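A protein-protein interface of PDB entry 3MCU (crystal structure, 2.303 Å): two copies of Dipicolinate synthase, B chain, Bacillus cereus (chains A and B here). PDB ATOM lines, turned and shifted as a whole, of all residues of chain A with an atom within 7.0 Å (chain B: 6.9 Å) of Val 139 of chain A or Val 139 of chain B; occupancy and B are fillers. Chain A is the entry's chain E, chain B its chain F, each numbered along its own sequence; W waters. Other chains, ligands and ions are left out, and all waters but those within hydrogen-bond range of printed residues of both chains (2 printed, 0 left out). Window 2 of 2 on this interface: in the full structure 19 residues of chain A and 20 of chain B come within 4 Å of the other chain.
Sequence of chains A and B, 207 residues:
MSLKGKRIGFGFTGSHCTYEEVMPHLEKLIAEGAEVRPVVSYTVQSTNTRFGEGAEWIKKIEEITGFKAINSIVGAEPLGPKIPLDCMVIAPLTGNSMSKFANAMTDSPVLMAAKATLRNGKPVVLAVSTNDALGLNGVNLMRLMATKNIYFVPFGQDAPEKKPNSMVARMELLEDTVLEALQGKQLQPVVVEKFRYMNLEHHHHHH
The backbone carbonyl oxygen (O) of Ala 133 of chain B sits close to the backbone NH (N) of Gly 138 of chain B.
The side-chain amide oxygen of Asn 140 of chain A sits at hydrogen-bond distance from the guanidinium group of Arg 143 of chain A (3.2 Å).
The backbone NH (N) of Gly 138 of chain A lies close to the backbone carbonyl oxygen (O) of Ala 133 of chain A, at 3.4 Å.
OD1 of Asn 140 of chain B lies within hydrogen-bond range of NH1 of Arg 143 of chain B.
Among the printed residues, pairs that only touch across the chains: Gly 135 of chain A with Ala 146 of chain B, Gly 138 of chain A with Met 142 of chain B, Val 139 of chain A with Val 139 of chain B, Val 139 of chain A with Met 142 of chain B, Val 139 of chain A with Arg 143 of chain B, Met 142 of chain A with Gly 138 of chain B, Met 142 of chain A with Val 139 of chain B, Met 142 of chain A with Met 142 of chain B, Arg 143 of chain A with Val 139 of chain B and Ala 146 of chain A with Gly 135 of chain B.
Of chain B, only Met 142 (3.3 Å) comes within 4 Å of Gly 138 of chain A.
Printed residues of chain A within 4 Å of Gly 135 of chain B: Ala 146.
Asn 137 of chain B touches none of the printed residues of chain A.
Val 139 of chain B touches just these residues of chain A: Val 139 (3.6 Å), Met 142 (3.7 Å) and Arg 143 (3.9 Å).
Printed residues of chain A within 4 Å of Arg 143 of chain B: Val 139 (3.8 Å).
The nearest residue of chain A that does not touch Val 139 of chain B is Gly 138 of chain A (5.7 Å).
Of the 14 printed residues of chain B, 6 touch a printed residue of chain A.
Hydrophobic or aromatic side chains of chain B that line the printed part of chain A: Val 139, Met 142 and Ala 146.
Hydrophobic or aromatic side chains of chain A within 4 Å of the printed part of chain B: Val 139, Met 142 and Ala 146.
Among the printed residues, 10 pairs touch across the chains.
Among the printed residues, no Asp or Glu carboxylate lies within 4 Å of a Lys or Arg side-chain nitrogen of the other chain.
Gly 135 of chain A touches Ala 146 of chain B, and with the chains exchanged Ala 146 of chain A touches Gly 135 of chain B.
Val 139 of chain A touches its own counterpart, Val 139 of chain B.
Val 139 of chain A touches Arg 143 of chain B, and with the chains exchanged Arg 143 of chain A touches Val 139 of chain B.
Met 142 of chain A touches its own counterpart, Met 142 of chain B.
Positions printed for both chains: 102, 132, 133, 135, 136, 137, 138, 139, 140, 141, 142, 143, 144 and 146.
Of the 10 pairs that touch across the chains among the printed residues, 10 have their exchanged pair printed and touching as well.
Water W2 lies within hydrogen-bond range of the backbone carbonyl oxygen of Gly 135 of chain B (2.8 Å), the backbone NH of Val 139 of chain B (3.0 Å), the backbone carbonyl oxygen of Met 142 of chain A (3.2 Å) and the backbone NH of Gly 138 of chain B (3.4 Å).
Water W1 lies within hydrogen-bond range of O of Gly 135 of chain A (2.8 Å), O of Met 142 of chain B (3.0 Å) and N of Val 139 of chain A (3.1 Å).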
ATOM      1  N   ALA A 102      13.529 -20.102  27.733  1.00  0.00           N
ATOM      2  CA  ALA A 102      13.560 -18.640  27.721  1.00  0.00           C
ATOM      3  C   ALA A 102      14.704 -18.077  28.567  1.00  0.00           C
ATOM      4  O   ALA A 102      15.205 -16.989  28.302  1.00  0.00           O
ATOM      5  CB  ALA A 102      12.212 -18.072  28.195  1.00  0.00           C
ATOM      6  N   ASP A 132      -0.393 -22.068  32.805  1.00  0.00           N
ATOM      7  CA  ASP A 132       0.016 -20.793  33.406  1.00  0.00           C
ATOM      8  C   ASP A 132       0.546 -19.808  32.349  1.00  0.00           C
ATOM      9  O   ASP A 132       1.281 -18.874  32.680  1.00  0.00           O
ATOM     10  CB  ASP A 132       1.103 -21.020  34.484  1.00  0.00           C
ATOM     11  CG  ASP A 132       2.349 -21.707  33.921  1.00  0.00           C
ATOM     12  OD1 ASP A 132       2.292 -22.167  32.752  1.00  0.00           O
ATOM     13  OD2 ASP A 132       3.389 -21.788  34.621  1.00  0.00           O
ATOM     14  N   ALA A 133       0.175 -20.015  31.084  1.00  0.00           N
ATOM     15  CA  ALA A 133       0.687 -19.189  29.988  1.00  0.00           C
ATOM     16  C   ALA A 133       0.294 -17.719  30.114  1.00  0.00           C
ATOM     17  O   ALA A 133       0.996 -16.837  29.637  1.00  0.00           O
ATOM     18  CB  ALA A 133       0.231 -19.742  28.637  1.00  0.00           C
ATOM     19  N   GLY A 135      -0.391 -16.667  33.099  1.00  0.00           N
ATOM     20  CA  GLY A 135       0.088 -16.408  34.439  1.00  0.00           C
ATOM     21  C   GLY A 135       1.562 -16.051  34.476  1.00  0.00           C
ATOM     22  O   GLY A 135       2.024 -15.174  33.746  1.00  0.00           O
ATOM     23  N   LEU A 136       2.302 -16.747  35.331  1.00  0.00           N
ATOM     24  CA  LEU A 136       3.703 -16.438  35.561  1.00  0.00           C
ATOM     25  C   LEU A 136       4.570 -16.759  34.342  1.00  0.00           C
ATOM     26  O   LEU A 136       5.643 -16.191  34.176  1.00  0.00           O
ATOM     27  CB  LEU A 136       4.205 -17.181  36.802  1.00  0.00           C
ATOM     28  CG  LEU A 136       3.941 -16.479  38.142  1.00  0.00           C
ATOM     29  CD1 LEU A 136       4.065 -17.430  39.320  1.00  0.00           C
ATOM     30  CD2 LEU A 136       4.885 -15.283  38.311  1.00  0.00           C
ATOM     31  N   ASN A 137       4.109 -17.660  33.480  1.00  0.00           N
ATOM     32  CA  ASN A 137       4.902 -18.028  32.303  1.00  0.00           C
ATOM     33  C   ASN A 137       4.747 -17.041  31.165  1.00  0.00           C
ATOM     34  O   ASN A 137       5.387 -17.171  30.122  1.00  0.00           O
ATOM     35  CB  ASN A 137       4.531 -19.422  31.817  1.00  0.00           C
ATOM     36  CG  ASN A 137       5.735 -20.331  31.691  1.00  0.00           C
ATOM     37  OD1 ASN A 137       6.864 -19.875  31.509  1.00  0.00           O
ATOM     38  ND2 ASN A 137       5.496 -21.639  31.796  1.00  0.00           N
ATOM     39  N   GLY A 138       3.865 -16.070  31.358  1.00  0.00           N
ATOM     40  CA  GLY A 138       3.512 -15.130  30.312  1.00  0.00           C
ATOM     41  C   GLY A 138       4.716 -14.334  29.862  1.00  0.00           C
ATOM     42  O   GLY A 138       4.917 -14.138  28.646  1.00  0.00           O
ATOM     43  N   VAL A 139       5.529 -13.881  30.821  1.00  0.00           N
ATOM     44  CA  VAL A 139       6.717 -13.124  30.465  1.00  0.00           C
ATOM     45  C   VAL A 139       7.700 -13.973  29.665  1.00  0.00           C
ATOM     46  O   VAL A 139       8.372 -13.467  28.775  1.00  0.00           O
ATOM     47  CB  VAL A 139       7.450 -12.493  31.687  1.00  0.00           C
ATOM     48  CG1 VAL A 139       6.709 -11.254  32.192  1.00  0.00           C
ATOM     49  CG2 VAL A 139       7.684 -13.535  32.796  1.00  0.00           C
ATOM     50  N   ASN A 140       7.784 -15.257  29.989  1.00  0.00           N
ATOM     51  CA  ASN A 140       8.715 -16.149  29.313  1.00  0.00           C
ATOM     52  C   ASN A 140       8.320 -16.371  27.869  1.00  0.00           C
ATOM     53  O   ASN A 140       9.171 -16.400  26.973  1.00  0.00           O
ATOM     54  CB  ASN A 140       8.785 -17.489  30.037  1.00  0.00           C
ATOM     55  CG  ASN A 140       9.515 -17.385  31.365  1.00  0.00           C
ATOM     56  OD1 ASN A 140      10.445 -16.605  31.491  1.00  0.00           O
ATOM     57  ND2 ASN A 140       9.095 -18.171  32.353  1.00  0.00           N
ATOM     58  N   LEU A 141       7.018 -16.529  27.660  1.00  0.00           N
ATOM     59  CA  LEU A 141       6.468 -16.806  26.352  1.00  0.00           C
ATOM     60  C   LEU A 141       6.740 -15.603  25.458  1.00  0.00           C
ATOM     61  O   LEU A 141       7.115 -15.749  24.296  1.00  0.00           O
ATOM     62  CB  LEU A 141       4.963 -17.087  26.469  1.00  0.00           C
ATOM     63  CG  LEU A 141       4.126 -17.515  25.265  1.00  0.00           C
ATOM     64  CD1 LEU A 141       2.794 -18.116  25.745  1.00  0.00           C
ATOM     65  CD2 LEU A 141       3.875 -16.354  24.324  1.00  0.00           C
ATOM     66  N   MET A 142       6.556 -14.408  26.015  1.00  0.00           N
ATOM     67  CA  MET A 142       6.765 -13.191  25.239  1.00  0.00           C
ATOM     68  C   MET A 142       8.246 -12.890  25.013  1.00  0.00           C
ATOM     69  O   MET A 142       8.585 -12.257  24.021  1.00  0.00           O
ATOM     70  CB  MET A 142       6.033 -11.994  25.857  1.00  0.00           C
ATOM     71  CG  MET A 142       4.518 -12.063  25.720  1.00  0.00           C
ATOM     72  SD  MET A 142       3.886 -12.143  23.839  1.00  0.00           S
ATOM     73  CE  MET A 142       1.966 -11.850  24.151  1.00  0.00           C
ATOM     74  N   ARG A 143       9.125 -13.326  25.918  1.00  0.00           N
ATOM     75  CA  ARG A 143      10.559 -13.115  25.693  1.00  0.00           C
ATOM     76  C   ARG A 143      10.924 -13.863  24.407  1.00  0.00           C
ATOM     77  O   ARG A 143      11.494 -13.292  23.497  1.00  0.00           O
ATOM     78  CB  ARG A 143      11.424 -13.552  26.893  1.00  0.00           C
ATOM     79  CG  ARG A 143      12.976 -13.530  26.648  1.00  0.00           C
ATOM     80  CD  ARG A 143      13.785 -13.503  27.990  1.00  0.00           C
ATOM     81  NE  ARG A 143      13.001 -12.760  28.970  1.00  0.00           N
ATOM     82  CZ  ARG A 143      12.482 -13.266  30.091  1.00  0.00           C
ATOM     83  NH1 ARG A 143      12.706 -14.534  30.461  1.00  0.00           N
ATOM     84  NH2 ARG A 143      11.737 -12.484  30.857  1.00  0.00           N
ATOM     85  N   LEU A 144      10.539 -15.134  24.343  1.00  0.00           N
ATOM     86  CA  LEU A 144      10.751 -15.985  23.180  1.00  0.00           C
ATOM     87  C   LEU A 144      10.143 -15.416  21.892  1.00  0.00           C
ATOM     88  O   LEU A 144      10.831 -15.279  20.897  1.00  0.00           O
ATOM     89  CB  LEU A 144      10.223 -17.399  23.458  1.00  0.00           C
ATOM     90  CG  LEU A 144      10.991 -18.130  24.565  1.00  0.00           C
ATOM     91  CD1 LEU A 144      10.273 -19.393  25.049  1.00  0.00           C
ATOM     92  CD2 LEU A 144      12.429 -18.454  24.138  1.00  0.00           C
ATOM     93  N   ALA A 146       9.797 -12.639  20.908  1.00  0.00           N
ATOM     94  CA  ALA A 146      10.491 -11.472  20.407  1.00  0.00           C
ATOM     95  C   ALA A 146      11.949 -11.767  20.051  1.00  0.00           C
ATOM     96  O   ALA A 146      12.629 -10.923  19.488  1.00  0.00           O
ATOM     97  CB  ALA A 146      10.407 -10.342  21.411  1.00  0.00           C
ATOM     98  N   ALA B 102       3.760  -0.696  33.239  1.00  0.00           N
ATOM     99  CA  ALA B 102       4.349  -1.961  33.656  1.00  0.00           C
ATOM    100  C   ALA B 102       5.607  -1.734  34.482  1.00  0.00           C
ATOM    101  O   ALA B 102       5.917  -2.518  35.361  1.00  0.00           O
ATOM    102  CB  ALA B 102       4.677  -2.833  32.451  1.00  0.00           C
ATOM    103  N   ASP B 132       3.425  -3.186  18.587  1.00  0.00           N
ATOM    104  CA  ASP B 132       4.553  -3.980  19.068  1.00  0.00           C
ATOM    105  C   ASP B 132       4.205  -4.900  20.250  1.00  0.00           C
ATOM    106  O   ASP B 132       5.097  -5.299  21.023  1.00  0.00           O
ATOM    107  CB  ASP B 132       5.740  -3.072  19.438  1.00  0.00           C
ATOM    108  CG  ASP B 132       5.401  -2.072  20.543  1.00  0.00           C
ATOM    109  OD1 ASP B 132       4.246  -2.076  21.050  1.00  0.00           O
ATOM    110  OD2 ASP B 132       6.285  -1.269  20.915  1.00  0.00           O
ATOM    111  N   ALA B 133       2.920  -5.234  20.389  1.00  0.00           N
ATOM    112  CA  ALA B 133       2.461  -6.078  21.487  1.00  0.00           C
ATOM    113  C   ALA B 133       3.134  -7.440  21.438  1.00  0.00           C
ATOM    114  O   ALA B 133       3.386  -8.054  22.474  1.00  0.00           O
ATOM    115  CB  ALA B 133       0.938  -6.239  21.461  1.00  0.00           C
ATOM    116  N   GLY B 135       6.025  -7.814  19.913  1.00  0.00           N
ATOM    117  CA  GLY B 135       7.451  -7.519  19.862  1.00  0.00           C
ATOM    118  C   GLY B 135       7.946  -7.122  21.246  1.00  0.00           C
ATOM    119  O   GLY B 135       7.571  -7.757  22.241  1.00  0.00           O
ATOM    120  N   LEU B 136       8.740  -6.055  21.322  1.00  0.00           N
ATOM    121  CA  LEU B 136       9.366  -5.655  22.584  1.00  0.00           C
ATOM    122  C   LEU B 136       8.376  -5.408  23.728  1.00  0.00           C
ATOM    123  O   LEU B 136       8.743  -5.530  24.891  1.00  0.00           O
ATOM    124  CB  LEU B 136      10.260  -4.426  22.387  1.00  0.00           C
ATOM    125  CG  LEU B 136      11.587  -4.669  21.668  1.00  0.00           C
ATOM    126  CD1 LEU B 136      12.155  -3.383  21.151  1.00  0.00           C
ATOM    127  CD2 LEU B 136      12.543  -5.350  22.618  1.00  0.00           C
ATOM    128  N   ASN B 137       7.127  -5.074  23.405  1.00  0.00           N
ATOM    129  CA  ASN B 137       6.142  -4.744  24.448  1.00  0.00           C
ATOM    130  C   ASN B 137       5.457  -5.967  25.006  1.00  0.00           C
ATOM    131  O   ASN B 137       4.660  -5.867  25.944  1.00  0.00           O
ATOM    132  CB  ASN B 137       5.068  -3.794  23.916  1.00  0.00           C
ATOM    133  CG  ASN B 137       4.966  -2.528  24.726  1.00  0.00           C
ATOM    134  OD1 ASN B 137       5.315  -2.505  25.911  1.00  0.00           O
ATOM    135  ND2 ASN B 137       4.500  -1.456  24.095  1.00  0.00           N
ATOM    136  N   GLY B 138       5.752  -7.122  24.419  1.00  0.00           N
ATOM    137  CA  GLY B 138       5.127  -8.367  24.833  1.00  0.00           C
ATOM    138  C   GLY B 138       5.336  -8.662  26.311  1.00  0.00           C
ATOM    139  O   GLY B 138       4.387  -9.024  27.029  1.00  0.00           O
ATOM    140  N   VAL B 139       6.577  -8.498  26.763  1.00  0.00           N
ATOM    141  CA  VAL B 139       6.958  -8.792  28.138  1.00  0.00           C
ATOM    142  C   VAL B 139       6.229  -7.884  29.110  1.00  0.00           C
ATOM    143  O   VAL B 139       5.847  -8.319  30.206  1.00  0.00           O
ATOM    144  CB  VAL B 139       8.502  -8.677  28.364  1.00  0.00           C
ATOM    145  CG1 VAL B 139       8.819  -8.656  29.840  1.00  0.00           C
ATOM    146  CG2 VAL B 139       9.219  -9.832  27.710  1.00  0.00           C
ATOM    147  N   ASN B 140       6.039  -6.624  28.726  1.00  0.00           N
ATOM    148  CA  ASN B 140       5.281  -5.685  29.563  1.00  0.00           C
ATOM    149  C   ASN B 140       3.795  -6.056  29.694  1.00  0.00           C
ATOM    150  O   ASN B 140       3.204  -6.003  30.781  1.00  0.00           O
ATOM    151  CB  ASN B 140       5.415  -4.279  29.005  1.00  0.00           C
ATOM    152  CG  ASN B 140       6.835  -3.781  29.070  1.00  0.00           C
ATOM    153  OD1 ASN B 140       7.543  -4.060  30.040  1.00  0.00           O
ATOM    154  ND2 ASN B 140       7.262  -3.041  28.054  1.00  0.00           N
ATOM    155  N   LEU B 141       3.194  -6.434  28.577  1.00  0.00           N
ATOM    156  CA  LEU B 141       1.791  -6.820  28.581  1.00  0.00           C
ATOM    157  C   LEU B 141       1.613  -8.007  29.513  1.00  0.00           C
ATOM    158  O   LEU B 141       0.677  -8.056  30.291  1.00  0.00           O
ATOM    159  CB  LEU B 141       1.324  -7.166  27.156  1.00  0.00           C
ATOM    160  CG  LEU B 141      -0.120  -7.605  26.929  1.00  0.00           C
ATOM    161  CD1 LEU B 141      -0.479  -7.441  25.453  1.00  0.00           C
ATOM    162  CD2 LEU B 141      -0.322  -9.038  27.355  1.00  0.00           C
ATOM    163  N   MET B 142       2.529  -8.965  29.439  1.00  0.00           N
ATOM    164  CA  MET B 142       2.373 -10.171  30.234  1.00  0.00           C
ATOM    165  C   MET B 142       2.702  -9.971  31.725  1.00  0.00           C
ATOM    166  O   MET B 142       2.135 -10.664  32.579  1.00  0.00           O
ATOM    167  CB  MET B 142       3.139 -11.334  29.619  1.00  0.00           C
ATOM    168  CG  MET B 142       2.507 -11.847  28.321  1.00  0.00           C
ATOM    169  SD  MET B 142       0.719 -12.595  28.602  1.00  0.00           S
ATOM    170  CE  MET B 142       0.386 -13.270  26.781  1.00  0.00           C
ATOM    171  N   ARG B 143       3.584  -9.020  32.034  1.00  0.00           N
ATOM    172  CA  ARG B 143       3.853  -8.667  33.423  1.00  0.00           C
ATOM    173  C   ARG B 143       2.571  -8.095  34.029  1.00  0.00           C
ATOM    174  O   ARG B 143       2.181  -8.467  35.137  1.00  0.00           O
ATOM    175  CB  ARG B 143       5.011  -7.668  33.525  1.00  0.00           C
ATOM    176  CG  ARG B 143       5.348  -7.206  34.946  1.00  0.00           C
ATOM    177  CD  ARG B 143       6.626  -6.350  34.936  1.00  0.00           C
ATOM    178  NE  ARG B 143       7.677  -6.983  34.140  1.00  0.00           N
ATOM    179  CZ  ARG B 143       8.257  -6.449  33.060  1.00  0.00           C
ATOM    180  NH1 ARG B 143       7.905  -5.238  32.612  1.00  0.00           N
ATOM    181  NH2 ARG B 143       9.198  -7.134  32.420  1.00  0.00           N
ATOM    182  N   LEU B 144       1.903  -7.224  33.268  1.00  0.00           N
ATOM    183  CA  LEU B 144       0.635  -6.638  33.675  1.00  0.00           C
ATOM    184  C   LEU B 144      -0.456  -7.694  33.842  1.00  0.00           C
ATOM    185  O   LEU B 144      -1.131  -7.714  34.869  1.00  0.00           O
ATOM    186  CB  LEU B 144       0.177  -5.555  32.690  1.00  0.00           C
ATOM    187  CG  LEU B 144       1.062  -4.303  32.680  1.00  0.00           C
ATOM    188  CD1 LEU B 144       0.792  -3.465  31.448  1.00  0.00           C
ATOM    189  CD2 LEU B 144       0.869  -3.480  33.949  1.00  0.00           C
ATOM    190  N   ALA B 146      -0.283 -10.592  34.719  1.00  0.00           N
ATOM    191  CA  ALA B 146      -0.020 -11.432  35.871  1.00  0.00           C
ATOM    192  C   ALA B 146      -0.088 -10.672  37.199  1.00  0.00           C
ATOM    193  O   ALA B 146      -0.019 -11.287  38.247  1.00  0.00           O
ATOM    194  CB  ALA B 146       1.356 -12.113  35.724  1.00  0.00           C
HETATM  195  O   HOH W   1       3.850 -13.046  33.329  1.00  0.00           O
HETATM  196  O   HOH W   2       8.449  -9.140  24.487  1.00  0.00           O
